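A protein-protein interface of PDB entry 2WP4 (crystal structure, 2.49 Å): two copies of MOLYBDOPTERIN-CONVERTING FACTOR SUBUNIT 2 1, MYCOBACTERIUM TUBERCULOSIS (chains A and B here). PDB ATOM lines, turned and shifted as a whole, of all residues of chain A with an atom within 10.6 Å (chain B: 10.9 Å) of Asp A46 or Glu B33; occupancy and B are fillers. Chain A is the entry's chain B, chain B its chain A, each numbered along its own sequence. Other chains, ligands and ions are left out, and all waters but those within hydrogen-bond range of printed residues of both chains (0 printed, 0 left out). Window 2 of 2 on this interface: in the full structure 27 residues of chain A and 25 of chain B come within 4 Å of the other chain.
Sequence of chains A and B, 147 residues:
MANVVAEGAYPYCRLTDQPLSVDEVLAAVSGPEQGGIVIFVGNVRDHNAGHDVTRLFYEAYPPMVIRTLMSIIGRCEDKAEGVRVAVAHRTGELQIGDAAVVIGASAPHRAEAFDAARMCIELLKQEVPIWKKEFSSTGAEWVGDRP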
ATOM      1  N   VAL A  41      13.353 -11.709 -10.500  1.00  0.00           N
ATOM      2  CA  VAL A  41      13.451 -13.054 -11.063  1.00  0.00           C
ATOM      3  C   VAL A  41      12.303 -13.865 -10.491  1.00  0.00           C
ATOM      4  O   VAL A  41      12.203 -14.028  -9.264  1.00  0.00           O
ATOM      5  CB  VAL A  41      14.781 -13.760 -10.665  1.00  0.00           C
ATOM      6  CG1 VAL A  41      14.893 -15.129 -11.317  1.00  0.00           C
ATOM      7  CG2 VAL A  41      15.996 -12.892 -10.999  1.00  0.00           C
ATOM      8  N   GLY A  42      11.438 -14.368 -11.375  1.00  0.00           N
ATOM      9  CA  GLY A  42      10.328 -15.234 -10.984  1.00  0.00           C
ATOM     10  C   GLY A  42      10.709 -16.674 -11.231  1.00  0.00           C
ATOM     11  O   GLY A  42      10.922 -17.072 -12.380  1.00  0.00           O
ATOM     12  N   ASN A  43      10.803 -17.447 -10.151  1.00  0.00           N
ATOM     13  CA  ASN A  43      11.266 -18.835 -10.205  1.00  0.00           C
ATOM     14  C   ASN A  43      10.163 -19.872 -10.042  1.00  0.00           C
ATOM     15  O   ASN A  43       9.150 -19.627  -9.384  1.00  0.00           O
ATOM     16  CB  ASN A  43      12.313 -19.110  -9.115  1.00  0.00           C
ATOM     17  CG  ASN A  43      13.635 -18.413  -9.365  1.00  0.00           C
ATOM     18  OD1 ASN A  43      14.095 -18.289 -10.503  1.00  0.00           O
ATOM     19  ND2 ASN A  43      14.263 -17.966  -8.291  1.00  0.00           N
ATOM     20  N   VAL A  44      10.390 -21.042 -10.633  1.00  0.00           N
ATOM     21  CA  VAL A  44       9.585 -22.225 -10.344  1.00  0.00           C
ATOM     22  C   VAL A  44       9.988 -22.764  -8.968  1.00  0.00           C
ATOM     23  O   VAL A  44      11.135 -23.168  -8.765  1.00  0.00           O
ATOM     24  CB  VAL A  44       9.762 -23.308 -11.434  1.00  0.00           C
ATOM     25  CG1 VAL A  44       9.131 -24.631 -11.011  1.00  0.00           C
ATOM     26  CG2 VAL A  44       9.162 -22.834 -12.750  1.00  0.00           C
ATOM     27  N   ARG A  45       9.055 -22.731  -8.020  1.00  0.00           N
ATOM     28  CA  ARG A  45       9.272 -23.335  -6.696  1.00  0.00           C
ATOM     29  C   ARG A  45       8.487 -24.645  -6.553  1.00  0.00           C
ATOM     30  O   ARG A  45       7.742 -25.019  -7.459  1.00  0.00           O
ATOM     31  CB  ARG A  45       8.930 -22.347  -5.571  1.00  0.00           C
ATOM     32  CG  ARG A  45       7.540 -21.763  -5.631  1.00  0.00           C
ATOM     33  CD  ARG A  45       7.237 -20.921  -4.407  1.00  0.00           C
ATOM     34  NE  ARG A  45       5.842 -20.495  -4.429  1.00  0.00           N
ATOM     35  CZ  ARG A  45       4.852 -21.121  -3.796  1.00  0.00           C
ATOM     36  NH1 ARG A  45       5.092 -22.198  -3.056  1.00  0.00           N
ATOM     37  NH2 ARG A  45       3.612 -20.661  -3.903  1.00  0.00           N
ATOM     38  N   ASP A  46       8.630 -25.336  -5.439  1.00  0.00           N
ATOM     39  CA  ASP A  46       7.912 -26.603  -5.296  1.00  0.00           C
ATOM     40  C   ASP A  46       6.810 -26.613  -4.265  1.00  0.00           C
ATOM     41  O   ASP A  46       6.853 -25.873  -3.299  1.00  0.00           O
ATOM     42  CB  ASP A  46       8.862 -27.746  -5.013  1.00  0.00           C
ATOM     43  CG  ASP A  46       9.402 -27.683  -3.656  1.00  0.00           C
ATOM     44  OD1 ASP A  46       9.289 -26.596  -3.080  1.00  0.00           O
ATOM     45  OD2 ASP A  46       9.922 -28.701  -3.180  1.00  0.00           O
ATOM     46  N   HIS A  47       5.796 -27.429  -4.539  1.00  0.00           N
ATOM     47  CA  HIS A  47       4.676 -27.682  -3.633  1.00  0.00           C
ATOM     48  C   HIS A  47       4.376 -29.186  -3.493  1.00  0.00           C
ATOM     49  O   HIS A  47       3.237 -29.588  -3.334  1.00  0.00           O
ATOM     50  CB  HIS A  47       3.449 -26.944  -4.133  1.00  0.00           C
ATOM     51  CG  HIS A  47       3.703 -26.109  -5.351  1.00  0.00           C
ATOM     52  ND1 HIS A  47       4.125 -24.802  -5.283  1.00  0.00           N
ATOM     53  CD2 HIS A  47       3.590 -26.398  -6.666  1.00  0.00           C
ATOM     54  CE1 HIS A  47       4.268 -24.326  -6.502  1.00  0.00           C
ATOM     55  NE2 HIS A  47       3.947 -25.273  -7.358  1.00  0.00           N
ATOM     56  N   ASN A  48       5.411 -30.005  -3.596  1.00  0.00           N
ATOM     57  CA  ASN A  48       5.340 -31.479  -3.573  1.00  0.00           C
ATOM     58  C   ASN A  48       4.461 -32.121  -4.652  1.00  0.00           C
ATOM     59  O   ASN A  48       4.144 -33.320  -4.578  1.00  0.00           O
ATOM     60  CB  ASN A  48       4.934 -31.988  -2.184  1.00  0.00           C
ATOM     61  CG  ASN A  48       6.081 -31.955  -1.190  1.00  0.00           C
ATOM     62  OD1 ASN A  48       6.878 -31.006  -1.165  1.00  0.00           O
ATOM     63  ND2 ASN A  48       6.166 -32.993  -0.353  1.00  0.00           N
ATOM     64  N   ASP A  52       7.864 -32.014  -9.467  1.00  0.00           N
ATOM     65  CA  ASP A  52       9.260 -31.593  -9.585  1.00  0.00           C
ATOM     66  C   ASP A  52       9.582 -30.913 -10.936  1.00  0.00           C
ATOM     67  O   ASP A  52      10.670 -30.347 -11.121  1.00  0.00           O
ATOM     68  CB  ASP A  52      10.205 -32.775  -9.295  1.00  0.00           C
ATOM     69  CG  ASP A  52      10.167 -33.852 -10.377  1.00  0.00           C
ATOM     70  OD1 ASP A  52       9.448 -34.862 -10.199  1.00  0.00           O
ATOM     71  OD2 ASP A  52      10.864 -33.696 -11.402  1.00  0.00           O
ATOM     72  N   VAL A  53       8.620 -30.958 -11.860  1.00  0.00           N
ATOM     73  CA  VAL A  53       8.765 -30.380 -13.201  1.00  0.00           C
ATOM     74  C   VAL A  53       7.554 -29.509 -13.556  1.00  0.00           C
ATOM     75  O   VAL A  53       6.417 -29.849 -13.220  1.00  0.00           O
ATOM     76  CB  VAL A  53       8.978 -31.508 -14.268  1.00  0.00           C
ATOM     77  CG1 VAL A  53       8.449 -31.112 -15.659  1.00  0.00           C
ATOM     78  CG2 VAL A  53      10.450 -31.911 -14.331  1.00  0.00           C
ATOM     79  N   THR A  54       7.804 -28.384 -14.227  1.00  0.00           N
ATOM     80  CA  THR A  54       6.728 -27.510 -14.690  1.00  0.00           C
ATOM     81  C   THR A  54       6.830 -27.252 -16.191  1.00  0.00           C
ATOM     82  O   THR A  54       7.887 -26.881 -16.702  1.00  0.00           O
ATOM     83  CB  THR A  54       6.704 -26.159 -13.928  1.00  0.00           C
ATOM     84  OG1 THR A  54       6.420 -26.383 -12.544  1.00  0.00           O
ATOM     85  CG2 THR A  54       5.633 -25.251 -14.482  1.00  0.00           C
ATOM     86  N   LEU A  94      10.591 -26.667 -17.424  1.00  0.00           N
ATOM     87  CA  LEU A  94      11.420 -26.004 -16.416  1.00  0.00           C
ATOM     88  C   LEU A  94      11.551 -26.832 -15.135  1.00  0.00           C
ATOM     89  O   LEU A  94      10.616 -27.522 -14.739  1.00  0.00           O
ATOM     90  CB  LEU A  94      10.858 -24.614 -16.085  1.00  0.00           C
ATOM     91  CG  LEU A  94      11.111 -23.418 -17.011  1.00  0.00           C
ATOM     92  CD1 LEU A  94      10.274 -23.470 -18.290  1.00  0.00           C
ATOM     93  CD2 LEU A  94      10.826 -22.127 -16.262  1.00  0.00           C
ATOM     94  N   GLN A  95      12.714 -26.736 -14.492  1.00  0.00           N
ATOM     95  CA  GLN A  95      12.997 -27.412 -13.223  1.00  0.00           C
ATOM     96  C   GLN A  95      12.699 -26.515 -12.020  1.00  0.00           C
ATOM     97  O   GLN A  95      12.660 -25.286 -12.148  1.00  0.00           O
ATOM     98  CB  GLN A  95      14.480 -27.821 -13.168  1.00  0.00           C
ATOM     99  CG  GLN A  95      14.930 -28.763 -14.279  1.00  0.00           C
ATOM    100  CD  GLN A  95      14.415 -30.168 -14.075  1.00  0.00           C
ATOM    101  OE1 GLN A  95      14.735 -30.812 -13.075  1.00  0.00           O
ATOM    102  NE2 GLN A  95      13.609 -30.655 -15.018  1.00  0.00           N
ATOM    103  N   ILE A  96      12.495 -27.137 -10.856  1.00  0.00           N
ATOM    104  CA  ILE A  96      12.467 -26.433  -9.572  1.00  0.00           C
ATOM    105  C   ILE A  96      13.740 -25.602  -9.471  1.00  0.00           C
ATOM    106  O   ILE A  96      14.846 -26.143  -9.593  1.00  0.00           O
ATOM    107  CB  ILE A  96      12.419 -27.425  -8.358  1.00  0.00           C
ATOM    108  CG1 ILE A  96      11.143 -28.282  -8.364  1.00  0.00           C
ATOM    109  CG2 ILE A  96      12.584 -26.691  -7.024  1.00  0.00           C
ATOM    110  CD1 ILE A  96       9.846 -27.492  -8.418  1.00  0.00           C
ATOM    111  N   GLY A  97      13.588 -24.295  -9.265  1.00  0.00           N
ATOM    112  CA  GLY A  97      14.733 -23.401  -9.193  1.00  0.00           C
ATOM    113  C   GLY A  97      14.959 -22.584 -10.455  1.00  0.00           C
ATOM    114  O   GLY A  97      15.641 -21.558 -10.408  1.00  0.00           O
ATOM    115  N   ASP A  98      14.395 -23.027 -11.581  1.00  0.00           N
ATOM    116  CA  ASP A  98      14.576 -22.334 -12.858  1.00  0.00           C
ATOM    117  C   ASP A  98      13.814 -21.011 -12.894  1.00  0.00           C
ATOM    118  O   ASP A  98      12.682 -20.912 -12.398  1.00  0.00           O
ATOM    119  CB  ASP A  98      14.136 -23.210 -14.045  1.00  0.00           C
ATOM    120  CG  ASP A  98      15.164 -24.279 -14.426  1.00  0.00           C
ATOM    121  OD1 ASP A  98      16.327 -24.218 -13.979  1.00  0.00           O
ATOM    122  OD2 ASP A  98      14.807 -25.189 -15.200  1.00  0.00           O
ATOM    123  N   LYS A 132       0.012 -23.482 -17.957  1.00  0.00           N
ATOM    124  CA  LYS A 132       0.897 -24.024 -16.915  1.00  0.00           C
ATOM    125  C   LYS A 132       0.381 -25.325 -16.315  1.00  0.00           C
ATOM    126  O   LYS A 132      -0.761 -25.394 -15.854  1.00  0.00           O
ATOM    127  CB  LYS A 132       1.114 -22.998 -15.794  1.00  0.00           C
ATOM    128  CG  LYS A 132       1.826 -23.551 -14.556  1.00  0.00           C
ATOM    129  CD  LYS A 132       2.341 -22.447 -13.635  1.00  0.00           C
ATOM    130  CE  LYS A 132       1.312 -22.046 -12.582  1.00  0.00           C
ATOM    131  NZ  LYS A 132       1.777 -20.862 -11.796  1.00  0.00           N
ATOM    132  N   GLU A 134       1.878 -28.781 -13.742  1.00  0.00           N
ATOM    133  CA  GLU A 134       2.919 -29.438 -12.956  1.00  0.00           C
ATOM    134  C   GLU A 134       2.921 -30.948 -13.160  1.00  0.00           C
ATOM    135  O   GLU A 134       1.866 -31.573 -13.266  1.00  0.00           O
ATOM    136  CB  GLU A 134       2.778 -29.092 -11.477  1.00  0.00           C
ATOM    137  CG  GLU A 134       3.422 -27.766 -11.109  1.00  0.00           C
ATOM    138  CD  GLU A 134       2.666 -27.027 -10.029  1.00  0.00           C
ATOM    139  OE1 GLU A 134       2.318 -27.650  -8.999  1.00  0.00           O
ATOM    140  OE2 GLU A 134       2.419 -25.817 -10.216  1.00  0.00           O
ATOM    141  N   PHE A 135       4.125 -31.514 -13.218  1.00  0.00           N
ATOM    142  CA  PHE A 135       4.352 -32.940 -13.499  1.00  0.00           C
ATOM    143  C   PHE A 135       5.258 -33.580 -12.441  1.00  0.00           C
ATOM    144  O   PHE A 135       5.779 -32.894 -11.552  1.00  0.00           O
ATOM    145  CB  PHE A 135       4.994 -33.119 -14.885  1.00  0.00           C
ATOM    146  CG  PHE A 135       4.012 -33.153 -16.023  1.00  0.00           C
ATOM    147  CD1 PHE A 135       3.709 -34.363 -16.656  1.00  0.00           C
ATOM    148  CD2 PHE A 135       3.405 -31.980 -16.478  1.00  0.00           C
ATOM    149  CE1 PHE A 135       2.801 -34.412 -17.726  1.00  0.00           C
ATOM    150  CE2 PHE A 135       2.489 -32.011 -17.544  1.00  0.00           C
ATOM    151  CZ  PHE A 135       2.188 -33.234 -18.171  1.00  0.00           C
ATOM    152  N   ALA B  27      23.016 -16.068  -5.637  1.00  0.00           N
ATOM    153  CA  ALA B  27      23.149 -17.429  -5.133  1.00  0.00           C
ATOM    154  C   ALA B  27      22.811 -17.532  -3.640  1.00  0.00           C
ATOM    155  O   ALA B  27      22.150 -18.479  -3.222  1.00  0.00           O
ATOM    156  CB  ALA B  27      24.547 -17.978  -5.419  1.00  0.00           C
ATOM    157  N   VAL B  29      20.698 -16.114  -1.946  1.00  0.00           N
ATOM    158  CA  VAL B  29      19.322 -15.763  -1.708  1.00  0.00           C
ATOM    159  C   VAL B  29      18.406 -16.750  -2.462  1.00  0.00           C
ATOM    160  O   VAL B  29      17.186 -16.732  -2.312  1.00  0.00           O
ATOM    161  CB  VAL B  29      19.157 -14.245  -2.079  1.00  0.00           C
ATOM    162  CG1 VAL B  29      18.089 -13.977  -3.109  1.00  0.00           C
ATOM    163  CG2 VAL B  29      19.034 -13.366  -0.821  1.00  0.00           C
ATOM    164  N   SER B  30      19.018 -17.650  -3.230  1.00  0.00           N
ATOM    165  CA  SER B  30      18.280 -18.657  -3.988  1.00  0.00           C
ATOM    166  C   SER B  30      17.945 -19.904  -3.169  1.00  0.00           C
ATOM    167  O   SER B  30      18.527 -20.151  -2.108  1.00  0.00           O
ATOM    168  CB  SER B  30      19.032 -19.033  -5.270  1.00  0.00           C
ATOM    169  OG  SER B  30      18.968 -17.955  -6.192  1.00  0.00           O
ATOM    170  N   GLY B  31      16.987 -20.677  -3.675  1.00  0.00           N
ATOM    171  CA  GLY B  31      16.496 -21.845  -2.981  1.00  0.00           C
ATOM    172  C   GLY B  31      15.223 -22.417  -3.577  1.00  0.00           C
ATOM    173  O   GLY B  31      14.420 -21.684  -4.156  1.00  0.00           O
ATOM    174  N   PRO B  32      15.022 -23.733  -3.409  1.00  0.00           N
ATOM    175  CA  PRO B  32      13.852 -24.464  -3.899  1.00  0.00           C
ATOM    176  C   PRO B  32      12.512 -23.766  -3.626  1.00  0.00           C
ATOM    177  O   PRO B  32      11.602 -23.860  -4.439  1.00  0.00           O
ATOM    178  CB  PRO B  32      13.921 -25.790  -3.123  1.00  0.00           C
ATOM    179  CG  PRO B  32      15.351 -25.988  -2.836  1.00  0.00           C
ATOM    180  CD  PRO B  32      15.957 -24.613  -2.677  1.00  0.00           C
ATOM    181  N   GLU B  33      12.398 -23.070  -2.497  1.00  0.00           N
ATOM    182  CA  GLU B  33      11.117 -22.494  -2.078  1.00  0.00           C
ATOM    183  C   GLU B  33      10.953 -21.000  -2.381  1.00  0.00           C
ATOM    184  O   GLU B  33       9.877 -20.444  -2.160  1.00  0.00           O
ATOM    185  CB  GLU B  33      10.879 -22.761  -0.591  1.00  0.00           C
ATOM    186  CG  GLU B  33      10.462 -24.206  -0.275  1.00  0.00           C
ATOM    187  CD  GLU B  33      10.991 -24.690   1.069  1.00  0.00           C
ATOM    188  OE1 GLU B  33      12.013 -24.131   1.551  1.00  0.00           O
ATOM    189  OE2 GLU B  33      10.396 -25.639   1.638  1.00  0.00           O
ATOM    190  N   GLN B  34      12.014 -20.358  -2.879  1.00  0.00           N
ATOM    191  CA  GLN B  34      11.981 -18.926  -3.187  1.00  0.00           C
ATOM    192  C   GLN B  34      11.430 -18.683  -4.593  1.00  0.00           C
ATOM    193  O   GLN B  34      12.141 -18.837  -5.587  1.00  0.00           O
ATOM    194  CB  GLN B  34      13.373 -18.283  -3.036  1.00  0.00           C
ATOM    195  CG  GLN B  34      14.129 -18.633  -1.749  1.00  0.00           C
ATOM    196  CD  GLN B  34      13.300 -18.442  -0.478  1.00  0.00           C
ATOM    197  OE1 GLN B  34      12.819 -19.411   0.103  1.00  0.00           O
ATOM    198  NE2 GLN B  34      13.141 -17.192  -0.042  1.00  0.00           N
ATOM    199  N   GLY B  35      10.156 -18.315  -4.672  1.00  0.00           N
ATOM    200  CA  GLY B  35       9.506 -18.062  -5.957  1.00  0.00           C
ATOM    201  C   GLY B  35       9.865 -16.704  -6.515  1.00  0.00           C
ATOM    202  O   GLY B  35       9.883 -16.516  -7.731  1.00  0.00           O
ATOM    203  N   GLY B  36      10.158 -15.755  -5.624  1.00  0.00           N
ATOM    204  CA  GLY B  36      10.457 -14.387  -6.019  1.00  0.00           C
ATOM    205  C   GLY B  36      11.788 -13.881  -5.496  1.00  0.00           C
ATOM    206  O   GLY B  36      12.101 -14.029  -4.309  1.00  0.00           O
ATOM    207  N   ILE B  37      12.571 -13.287  -6.396  1.00  0.00           N
ATOM    208  CA  ILE B  37      13.858 -12.689  -6.058  1.00  0.00           C
ATOM    209  C   ILE B  37      13.937 -11.276  -6.625  1.00  0.00           C
ATOM    210  O   ILE B  37      13.756 -11.056  -7.838  1.00  0.00           O
ATOM    211  CB  ILE B  37      15.056 -13.510  -6.601  1.00  0.00           C
ATOM    212  CG1 ILE B  37      15.005 -14.962  -6.092  1.00  0.00           C
ATOM    213  CG2 ILE B  37      16.399 -12.817  -6.242  1.00  0.00           C
ATOM    214  CD1 ILE B  37      16.074 -15.857  -6.677  1.00  0.00           C
ATOM    215  N   GLU B  81       7.687 -14.807   6.638  1.00  0.00           N
ATOM    216  CA  GLU B  81       8.300 -16.135   6.617  1.00  0.00           C
ATOM    217  C   GLU B  81       8.980 -16.459   5.281  1.00  0.00           C
ATOM    218  O   GLU B  81       8.461 -16.131   4.212  1.00  0.00           O
ATOM    219  CB  GLU B  81       7.279 -17.214   6.975  1.00  0.00           C
ATOM    220  CG  GLU B  81       7.878 -18.457   7.665  1.00  0.00           C
ATOM    221  CD  GLU B  81       8.568 -18.130   8.994  1.00  0.00           C
ATOM    222  OE1 GLU B  81       9.737 -17.671   8.978  1.00  0.00           O
ATOM    223  OE2 GLU B  81       7.939 -18.336  10.053  1.00  0.00           O
ATOM    224  N   GLY B  82      10.153 -17.085   5.366  1.00  0.00           N
ATOM    225  CA  GLY B  82      10.904 -17.535   4.198  1.00  0.00           C
ATOM    226  C   GLY B  82      11.647 -16.435   3.466  1.00  0.00           C
ATOM    227  O   GLY B  82      12.040 -16.610   2.307  1.00  0.00           O
ATOM    228  N   VAL B  83      11.846 -15.300   4.131  1.00  0.00           N
ATOM    229  CA  VAL B  83      12.511 -14.159   3.508  1.00  0.00           C
ATOM    230  C   VAL B  83      14.023 -14.194   3.733  1.00  0.00           C
ATOM    231  O   VAL B  83      14.485 -14.229   4.869  1.00  0.00           O
ATOM    232  CB  VAL B  83      11.921 -12.804   3.988  1.00  0.00           C
ATOM    233  CG1 VAL B  83      12.752 -11.629   3.464  1.00  0.00           C
ATOM    234  CG2 VAL B  83      10.480 -12.661   3.541  1.00  0.00           C
ATOM    235  N   ARG B  84      14.782 -14.182   2.643  1.00  0.00           N
ATOM    236  CA  ARG B  84      16.238 -14.195   2.712  1.00  0.00           C
ATOM    237  C   ARG B  84      16.804 -12.923   2.124  1.00  0.00           C
ATOM    238  O   ARG B  84      16.379 -12.490   1.055  1.00  0.00           O
ATOM    239  CB  ARG B  84      16.801 -15.407   1.975  1.00  0.00           C
ATOM    240  CG  ARG B  84      16.401 -16.717   2.609  1.00  0.00           C
ATOM    241  CD  ARG B  84      16.909 -17.895   1.831  1.00  0.00           C
ATOM    242  NE  ARG B  84      16.327 -19.119   2.373  1.00  0.00           N
ATOM    243  CZ  ARG B  84      16.410 -20.319   1.803  1.00  0.00           C
ATOM    244  NH1 ARG B  84      17.058 -20.474   0.647  1.00  0.00           N
ATOM    245  NH2 ARG B  84      15.841 -21.362   2.397  1.00  0.00           N
ATOM    246  N   ALA B 105      17.000  -9.919  -2.134  1.00  0.00           N
ATOM    247  CA  ALA B 105      15.963 -10.400  -1.231  1.00  0.00           C
ATOM    248  C   ALA B 105      15.094 -11.391  -1.978  1.00  0.00           C
ATOM    249  O   ALA B 105      14.709 -11.143  -3.124  1.00  0.00           O
ATOM    250  CB  ALA B 105      15.116  -9.246  -0.696  1.00  0.00           C
ATOM    251  N   SER B 106      14.797 -12.511  -1.318  1.00  0.00           N
ATOM    252  CA  SER B 106      13.930 -13.534  -1.874  1.00  0.00           C
ATOM    253  C   SER B 106      12.840 -13.922  -0.886  1.00  0.00           C
ATOM    254  O   SER B 106      12.968 -13.686   0.320  1.00  0.00           O
ATOM    255  CB  SER B 106      14.735 -14.765  -2.289  1.00  0.00           C
ATOM    256  OG  SER B 106      15.257 -15.440  -1.157  1.00  0.00           O
ATOM    257  N   ALA B 107      11.773 -14.524  -1.411  1.00  0.00           N
ATOM    258  CA  ALA B 107      10.628 -14.948  -0.615  1.00  0.00           C
ATOM    259  C   ALA B 107       9.838 -15.988  -1.413  1.00  0.00           C
ATOM    260  O   ALA B 107      10.024 -16.095  -2.628  1.00  0.00           O
ATOM    261  CB  ALA B 107       9.746 -13.746  -0.267  1.00  0.00           C
ATOM    262  N   PRO B 108       8.973 -16.774  -0.742  1.00  0.00           N
ATOM    263  CA  PRO B 108       8.106 -17.659  -1.521  1.00  0.00           C
ATOM    264  C   PRO B 108       7.373 -16.894  -2.625  1.00  0.00           C
ATOM    265  O   PRO B 108       7.299 -17.374  -3.758  1.00  0.00           O
ATOM    266  CB  PRO B 108       7.119 -18.193  -0.470  1.00  0.00           C
ATOM    267  CG  PRO B 108       7.928 -18.249   0.787  1.00  0.00           C
ATOM    268  CD  PRO B 108       8.884 -17.056   0.708  1.00  0.00           C
ATOM    269  N   HIS B 109       6.877 -15.701  -2.295  1.00  0.00           N
ATOM    270  CA  HIS B 109       6.097 -14.880  -3.224  1.00  0.00           C
ATOM    271  C   HIS B 109       6.748 -13.513  -3.481  1.00  0.00           C
ATOM    272  O   HIS B 109       7.490 -12.999  -2.642  1.00  0.00           O
ATOM    273  CB  HIS B 109       4.670 -14.698  -2.707  1.00  0.00           C
ATOM    274  CG  HIS B 109       3.956 -15.986  -2.424  1.00  0.00           C
ATOM    275  ND1 HIS B 109       3.485 -16.815  -3.423  1.00  0.00           N
ATOM    276  CD2 HIS B 109       3.612 -16.579  -1.253  1.00  0.00           C
ATOM    277  CE1 HIS B 109       2.888 -17.860  -2.880  1.00  0.00           C
ATOM    278  NE2 HIS B 109       2.951 -17.743  -1.564  1.00  0.00           N
ATOM    279  N   ARG B 110       6.444 -12.921  -4.633  1.00  0.00           N
ATOM    280  CA  ARG B 110       7.110 -11.697  -5.073  1.00  0.00           C
ATOM    281  C   ARG B 110       6.882 -10.468  -4.186  1.00  0.00           C
ATOM    282  O   ARG B 110       7.774  -9.627  -4.071  1.00  0.00           O
ATOM    283  CB  ARG B 110       6.757 -11.368  -6.533  1.00  0.00           C
ATOM    284  CG  ARG B 110       5.314 -10.931  -6.762  1.00  0.00           C
ATOM    285  CD  ARG B 110       5.094 -10.568  -8.215  1.00  0.00           C
ATOM    286  NE  ARG B 110       3.693 -10.339  -8.551  1.00  0.00           N
ATOM    287  CZ  ARG B 110       2.768 -11.294  -8.642  1.00  0.00           C
ATOM    288  NH1 ARG B 110       3.085 -12.563  -8.387  1.00  0.00           N
ATOM    289  NH2 ARG B 110       1.520 -10.976  -8.982  1.00  0.00           N
ATOM    290  N   GLU B 112       6.706 -10.142  -0.977  1.00  0.00           N
ATOM    291  CA  GLU B 112       7.584 -10.109   0.189  1.00  0.00           C
ATOM    292  C   GLU B 112       9.042  -9.860  -0.181  1.00  0.00           C
ATOM    293  O   GLU B 112       9.792  -9.294   0.616  1.00  0.00           O
ATOM    294  CB  GLU B 112       7.429 -11.385   1.028  1.00  0.00           C
ATOM    295  CG  GLU B 112       6.156 -11.434   1.893  1.00  0.00           C
ATOM    296  CD  GLU B 112       4.857 -11.531   1.086  1.00  0.00           C
ATOM    297  OE1 GLU B 112       4.847 -12.142  -0.012  1.00  0.00           O
ATOM    298  OE2 GLU B 112       3.831 -10.998   1.563  1.00  0.00           O
ATOM    299  N   ALA B 113       9.432 -10.264  -1.390  1.00  0.00           N
ATOM    300  CA  ALA B 113      10.781 -10.014  -1.889  1.00  0.00           C
ATOM    301  C   ALA B 113      10.947  -8.540  -2.260  1.00  0.00           C
ATOM    302  O   ALA B 113      11.998  -7.937  -1.991  1.00  0.00           O
ATOM    303  CB  ALA B 113      11.093 -10.905  -3.084  1.00  0.00           C
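Gly B36 touches Val A41 (CA to O, 3.7 Å).
CA of Gly A42 touches O of Gly B35, 3.5 Å away.
Asn A43 touches Gln B34.
Ile B37 touches Asn A43.
Pro B32 touches Arg A45 (O to CB, 3.3 Å).
N of Gly B35 touches CD of Arg A45, at 3.9 Å.
Arg A45 touches Pro B108.
His B109 touches Arg A45 (CE1 to NH2, 3.1 Å).
OD1 of Asp A46 touches CG of Glu B33 (3.9 Å).
Pro B32 touches Ile A96 (O to CG2, 3.96 Å).
Printed residues of chain A that touch a printed residue of chain B: Val A41, Gly A42, Asn A43, Arg A45, Asp A46 and Ile A96.
Among the printed residues, no Asp or Glu carboxylate lies within 4 Å of a Lys or Arg side-chain nitrogen of the other chain.
The backbone carbonyl oxygen of Pro B32 is in hydrogen-bond range of the backbone NH of Asp A46, at 3.5 Å.
O of Gly B35 is in hydrogen-bond range of N of Asn A43, 2.8 Å away.
N of Val A41 lies within hydrogen-bond range of O of Ile B37 (2.8 Å).
NE2 of Gln B34 lies within hydrogen-bond range of O of Gly B82 (2.7 Å).
The side-chain amide nitrogen of Gln B34 is in hydrogen-bond range of the side-chain hydroxyl of Ser B106, 3.0 Å away.
The backbone NH (N) of Ala B107 lies close to the side-chain amide nitrogen (NE2) of Gln B34 (3.3 Å).
The backbone NH (N) of Gly B35 sits at hydrogen-bond distance from the backbone carbonyl oxygen (O) of Ala B107, at 3.0 Å.
The backbone carbonyl oxygen (O) of Pro B108 lies within hydrogen-bond range of the backbone NH (N) of Gly B35, at 3.1 Å.
N of Ala B107 is in hydrogen-bond range of O of Gly B36 (3.0 Å).
No position is printed for both chains.
Of the 15 pairs that touch across the chains among the printed residues, none has its exchanged pair printed and touching as well.
Of the printed residues of chain B, Gly A42 touches Gly B35.
Of the printed residues of chain B, Asn A43 touches Gln B34, Gly B35 and Ile B37.
Arg A45 touches just these residues of chain B: Pro B32 (3.3 Å), Glu B33 (3.5 Å), Gly B35 (3.9 Å), Pro B108 (3.5 Å) and His B109 (3.1 Å).
Asp A46 touches just these residues of chain B: Pro B32 (3.5 Å) and Glu B33 (3.9 Å).
No residue of chain B comes within 4 Å of His A47.
No residue of chain A comes within 4 Å of Gly B31.
Pro B32 touches just these residues of chain A: Arg A45 (3.3 Å), Asp A46 (3.5 Å) and Ile A96 (3.96 Å).
Gln B34 touches one residue of chain A.
Of the printed residues of chain A, Gly B36 touches Val A41 (3.7 Å).
Ala B105 touches none of the printed residues of chain A.
Pro B108 touches just one residue of chain A: Arg A45.
Of the printed residues of chain A, His B109 touches Arg A45.
Arg B110 touches none of the printed residues of chain A.
The nearest residue of chain B that does not touch Asp A46 is Gln B34 (6.5 Å).
The nearest printed residue of chain B that does not touch Gly A42 is Gly B36 (5.0 Å).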
